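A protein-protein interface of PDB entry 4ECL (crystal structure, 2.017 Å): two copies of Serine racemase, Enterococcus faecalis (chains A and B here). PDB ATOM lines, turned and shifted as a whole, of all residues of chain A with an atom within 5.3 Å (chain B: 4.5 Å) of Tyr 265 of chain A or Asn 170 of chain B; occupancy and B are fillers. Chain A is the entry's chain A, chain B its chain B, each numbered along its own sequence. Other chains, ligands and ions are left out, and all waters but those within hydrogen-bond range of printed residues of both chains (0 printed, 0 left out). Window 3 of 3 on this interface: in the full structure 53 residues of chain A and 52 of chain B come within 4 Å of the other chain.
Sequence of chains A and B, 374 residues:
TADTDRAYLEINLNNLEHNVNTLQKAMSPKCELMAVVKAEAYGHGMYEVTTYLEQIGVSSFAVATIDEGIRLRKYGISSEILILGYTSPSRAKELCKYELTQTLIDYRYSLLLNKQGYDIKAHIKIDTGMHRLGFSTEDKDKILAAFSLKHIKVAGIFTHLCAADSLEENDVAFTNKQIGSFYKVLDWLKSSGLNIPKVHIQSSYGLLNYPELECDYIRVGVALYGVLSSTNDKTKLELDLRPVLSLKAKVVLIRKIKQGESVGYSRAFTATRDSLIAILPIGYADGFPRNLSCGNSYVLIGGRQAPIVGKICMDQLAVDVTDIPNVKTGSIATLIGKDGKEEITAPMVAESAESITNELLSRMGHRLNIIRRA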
ATOM      1  N   SER A 262      16.782  20.569 -19.205  1.00  0.00           N
ATOM      2  CA  SER A 262      18.015  19.875 -18.854  1.00  0.00           C
ATOM      3  C   SER A 262      18.116  19.602 -17.361  1.00  0.00           C
ATOM      4  O   SER A 262      17.197  19.900 -16.594  1.00  0.00           O
ATOM      5  CB  SER A 262      19.235  20.688 -19.288  1.00  0.00           C
ATOM      6  OG  SER A 262      20.431  19.959 -19.032  1.00  0.00           O
ATOM      7  N   VAL A 263      19.243  19.027 -16.958  1.00  0.00           N
ATOM      8  CA  VAL A 263      19.595  18.920 -15.551  1.00  0.00           C
ATOM      9  C   VAL A 263      20.977  19.538 -15.363  1.00  0.00           C
ATOM     10  O   VAL A 263      21.942  19.139 -16.027  1.00  0.00           O
ATOM     11  CB  VAL A 263      19.611  17.462 -15.057  1.00  0.00           C
ATOM     12  CG1 VAL A 263      20.090  17.391 -13.605  1.00  0.00           C
ATOM     13  CG2 VAL A 263      18.227  16.829 -15.204  1.00  0.00           C
ATOM     14  N   GLY A 264      21.063  20.520 -14.470  1.00  0.00           N
ATOM     15  CA  GLY A 264      22.303  21.250 -14.251  1.00  0.00           C
ATOM     16  C   GLY A 264      22.705  22.056 -15.470  1.00  0.00           C
ATOM     17  O   GLY A 264      23.880  22.369 -15.652  1.00  0.00           O
ATOM     18  N   TYR A 265      21.713  22.378 -16.303  1.00  0.00           N
ATOM     19  CA  TYR A 265      21.879  23.065 -17.600  1.00  0.00           C
ATOM     20  C   TYR A 265      23.002  22.586 -18.536  1.00  0.00           C
ATOM     21  O   TYR A 265      23.115  23.065 -19.665  1.00  0.00           O
ATOM     22  CB  TYR A 265      21.925  24.597 -17.457  1.00  0.00           C
ATOM     23  CG  TYR A 265      21.795  25.305 -18.798  1.00  0.00           C
ATOM     24  CD1 TYR A 265      20.673  25.103 -19.601  1.00  0.00           C
ATOM     25  CD2 TYR A 265      22.808  26.128 -19.284  1.00  0.00           C
ATOM     26  CE1 TYR A 265      20.549  25.723 -20.831  1.00  0.00           C
ATOM     27  CE2 TYR A 265      22.692  26.755 -20.521  1.00  0.00           C
ATOM     28  CZ  TYR A 265      21.558  26.547 -21.286  1.00  0.00           C
ATOM     29  OH  TYR A 265      21.427  27.159 -22.513  1.00  0.00           O
ATOM     30  N   SER A 266      23.826  21.650 -18.084  1.00  0.00           N
ATOM     31  CA  SER A 266      24.838  21.089 -18.963  1.00  0.00           C
ATOM     32  C   SER A 266      24.150  20.586 -20.220  1.00  0.00           C
ATOM     33  O   SER A 266      23.251  19.747 -20.161  1.00  0.00           O
ATOM     34  CB  SER A 266      25.596  19.943 -18.294  1.00  0.00           C
ATOM     35  OG  SER A 266      24.759  18.809 -18.111  1.00  0.00           O
ATOM     36  N   ARG A 267      24.581  21.113 -21.360  1.00  0.00           N
ATOM     37  CA  ARG A 267      24.127  20.650 -22.670  1.00  0.00           C
ATOM     38  C   ARG A 267      24.356  19.138 -22.833  1.00  0.00           C
ATOM     39  O   ARG A 267      24.006  18.538 -23.850  1.00  0.00           O
ATOM     40  CB  ARG A 267      24.807  21.454 -23.791  1.00  0.00           C
ATOM     41  CG  ARG A 267      26.285  21.133 -24.051  1.00  0.00           C
ATOM     42  CD  ARG A 267      27.201  21.461 -22.871  1.00  0.00           C
ATOM     43  NE  ARG A 267      26.898  22.754 -22.266  1.00  0.00           N
ATOM     44  CZ  ARG A 267      27.442  23.905 -22.647  1.00  0.00           C
ATOM     45  NH1 ARG A 267      28.322  23.929 -23.641  1.00  0.00           N
ATOM     46  NH2 ARG A 267      27.104  25.034 -22.036  1.00  0.00           N
ATOM     47  N   GLY B 129      16.516  26.411 -12.349  1.00  0.00           N
ATOM     48  CA  GLY B 129      16.867  25.873 -13.651  1.00  0.00           C
ATOM     49  C   GLY B 129      17.792  24.668 -13.594  1.00  0.00           C
ATOM     50  O   GLY B 129      17.889  23.909 -14.557  1.00  0.00           O
ATOM     51  N   CYS B 162      23.908  27.731 -12.723  1.00  0.00           N
ATOM     52  CA  CYS B 162      24.429  26.597 -13.494  1.00  0.00           C
ATOM     53  C   CYS B 162      25.681  26.906 -14.300  1.00  0.00           C
ATOM     54  O   CYS B 162      26.590  26.084 -14.380  1.00  0.00           O
ATOM     55  CB  CYS B 162      23.354  26.044 -14.428  1.00  0.00           C
ATOM     56  SG  CYS B 162      21.986  25.246 -13.572  1.00  0.00           S
ATOM     57  N   GLU B 168      29.663  32.725 -22.568  1.00  0.00           N
ATOM     58  CA  GLU B 168      28.884  32.385 -23.755  1.00  0.00           C
ATOM     59  C   GLU B 168      27.461  32.937 -23.608  1.00  0.00           C
ATOM     60  O   GLU B 168      26.911  32.987 -22.505  1.00  0.00           O
ATOM     61  CB  GLU B 168      28.860  30.865 -23.973  1.00  0.00           C
ATOM     62  CG  GLU B 168      30.246  30.242 -24.177  1.00  0.00           C
ATOM     63  CD  GLU B 168      30.242  28.717 -24.073  1.00  0.00           C
ATOM     64  OE1 GLU B 168      29.211  28.089 -24.406  1.00  0.00           O
ATOM     65  OE2 GLU B 168      31.272  28.145 -23.652  1.00  0.00           O
ATOM     66  N   GLU B 169      26.872  33.360 -24.719  1.00  0.00           N
ATOM     67  CA  GLU B 169      25.575  34.015 -24.668  1.00  0.00           C
ATOM     68  C   GLU B 169      24.475  33.074 -24.179  1.00  0.00           C
ATOM     69  O   GLU B 169      23.493  33.520 -23.584  1.00  0.00           O
ATOM     70  CB  GLU B 169      25.211  34.611 -26.028  1.00  0.00           C
ATOM     71  CG  GLU B 169      24.520  33.652 -26.970  1.00  0.00           C
ATOM     72  CD  GLU B 169      24.264  34.269 -28.319  1.00  0.00           C
ATOM     73  OE1 GLU B 169      23.158  34.070 -28.860  1.00  0.00           O
ATOM     74  OE2 GLU B 169      25.170  34.954 -28.840  1.00  0.00           O
ATOM     75  N   ASN B 170      24.642  31.778 -24.421  1.00  0.00           N
ATOM     76  CA  ASN B 170      23.672  30.797 -23.941  1.00  0.00           C
ATOM     77  C   ASN B 170      23.672  30.737 -22.424  1.00  0.00           C
ATOM     78  O   ASN B 170      22.617  30.725 -21.785  1.00  0.00           O
ATOM     79  CB  ASN B 170      23.971  29.414 -24.516  1.00  0.00           C
ATOM     80  CG  ASN B 170      23.297  29.184 -25.851  1.00  0.00           C
ATOM     81  OD1 ASN B 170      22.692  30.097 -26.421  1.00  0.00           O
ATOM     82  ND2 ASN B 170      23.396  27.960 -26.361  1.00  0.00           N
ATOM     83  N   ASP B 171      24.878  30.724 -21.865  1.00  0.00           N
ATOM     84  CA  ASP B 171      25.091  30.621 -20.430  1.00  0.00           C
ATOM     85  C   ASP B 171      24.791  31.934 -19.714  1.00  0.00           C
ATOM     86  O   ASP B 171      24.300  31.928 -18.579  1.00  0.00           O
ATOM     87  CB  ASP B 171      26.526  30.176 -20.162  1.00  0.00           C
ATOM     88  CG  ASP B 171      26.873  28.884 -20.883  1.00  0.00           C
ATOM     89  OD1 ASP B 171      26.052  27.940 -20.833  1.00  0.00           O
ATOM     90  OD2 ASP B 171      27.948  28.821 -21.517  1.00  0.00           O
ATOM     91  N   VAL B 172      25.084  33.055 -20.377  1.00  0.00           N
ATOM     92  CA  VAL B 172      24.719  34.362 -19.844  1.00  0.00           C
ATOM     93  C   VAL B 172      23.207  34.504 -19.729  1.00  0.00           C
ATOM     94  O   VAL B 172      22.696  34.822 -18.656  1.00  0.00           O
ATOM     95  CB  VAL B 172      25.306  35.527 -20.673  1.00  0.00           C
ATOM     96  CG1 VAL B 172      24.589  36.828 -20.357  1.00  0.00           C
ATOM     97  CG2 VAL B 172      26.794  35.660 -20.396  1.00  0.00           C
ATOM     98  N   ALA B 173      22.498  34.255 -20.830  1.00  0.00           N
ATOM     99  CA  ALA B 173      21.039  34.319 -20.828  1.00  0.00           C
ATOM    100  C   ALA B 173      20.443  33.345 -19.813  1.00  0.00           C
ATOM    101  O   ALA B 173      19.476  33.670 -19.131  1.00  0.00           O
ATOM    102  CB  ALA B 173      20.480  34.056 -22.223  1.00  0.00           C
ATOM    103  N   PHE B 174      21.027  32.155 -19.698  1.00  0.00           N
ATOM    104  CA  PHE B 174      20.526  31.193 -18.723  1.00  0.00           C
ATOM    105  C   PHE B 174      20.806  31.660 -17.295  1.00  0.00           C
ATOM    106  O   PHE B 174      19.988  31.473 -16.398  1.00  0.00           O
ATOM    107  CB  PHE B 174      21.105  29.793 -18.952  1.00  0.00           C
ATOM    108  CG  PHE B 174      20.345  28.703 -18.238  1.00  0.00           C
ATOM    109  CD1 PHE B 174      19.244  28.104 -18.833  1.00  0.00           C
ATOM    110  CD2 PHE B 174      20.716  28.295 -16.967  1.00  0.00           C
ATOM    111  CE1 PHE B 174      18.532  27.103 -18.177  1.00  0.00           C
ATOM    112  CE2 PHE B 174      20.012  27.301 -16.307  1.00  0.00           C
ATOM    113  CZ  PHE B 174      18.918  26.701 -16.914  1.00  0.00           C
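NH2 of Arg 267 of chain A lies within salt-bridge range of OD1 of Asp 171 of chain B, 3.3 Å away.
Of the printed residues of chain B, Gly 264 of chain A touches Cys 162 (3.8 Å). Tyr 265 of chain A touches just these residues of chain B: Cys 162 (3.6 Å), Asn 170 (3.8 Å), Asp 171 (3.6 Å) and Phe 174 (3.3 Å). Ser 266 of chain A touches none of the printed residues of chain B. Glu 169 of chain B touches none of the printed residues of chain A. Asn 170 of chain B touches one residue of chain A. Of the printed residues of chain A, Asp 171 of chain B touches Tyr 265 and Arg 267.
Of the 9 printed residues of chain B, 4 touch a printed residue of chain A. Hydrophobic or aromatic side chains of chain B that line the printed part of chain A: Phe 174. Along chain B the printed residues that touch a printed residue of chain A span positions 162 to 174. Hydrophobic or aromatic side chains of chain A that line the printed part of chain B: Tyr 265. Among the printed residues, 6 pairs touch across the chains.
No position is printed for both chains.
Gly 264 of chain A touches Cys 162 of chain B (C to SG, 3.8 Å). Cys 162 of chain B touches Tyr 265 of chain A (CB to CB, 3.6 Å). O of Asn 170 of chain B touches OH of Tyr 265 of chain A (3.8 Å). Tyr 265 of chain A touches Asp 171 of chain B. CE1 of Phe 174 of chain B touches CD1 of Tyr 265 of chain A, 3.3 Å away.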
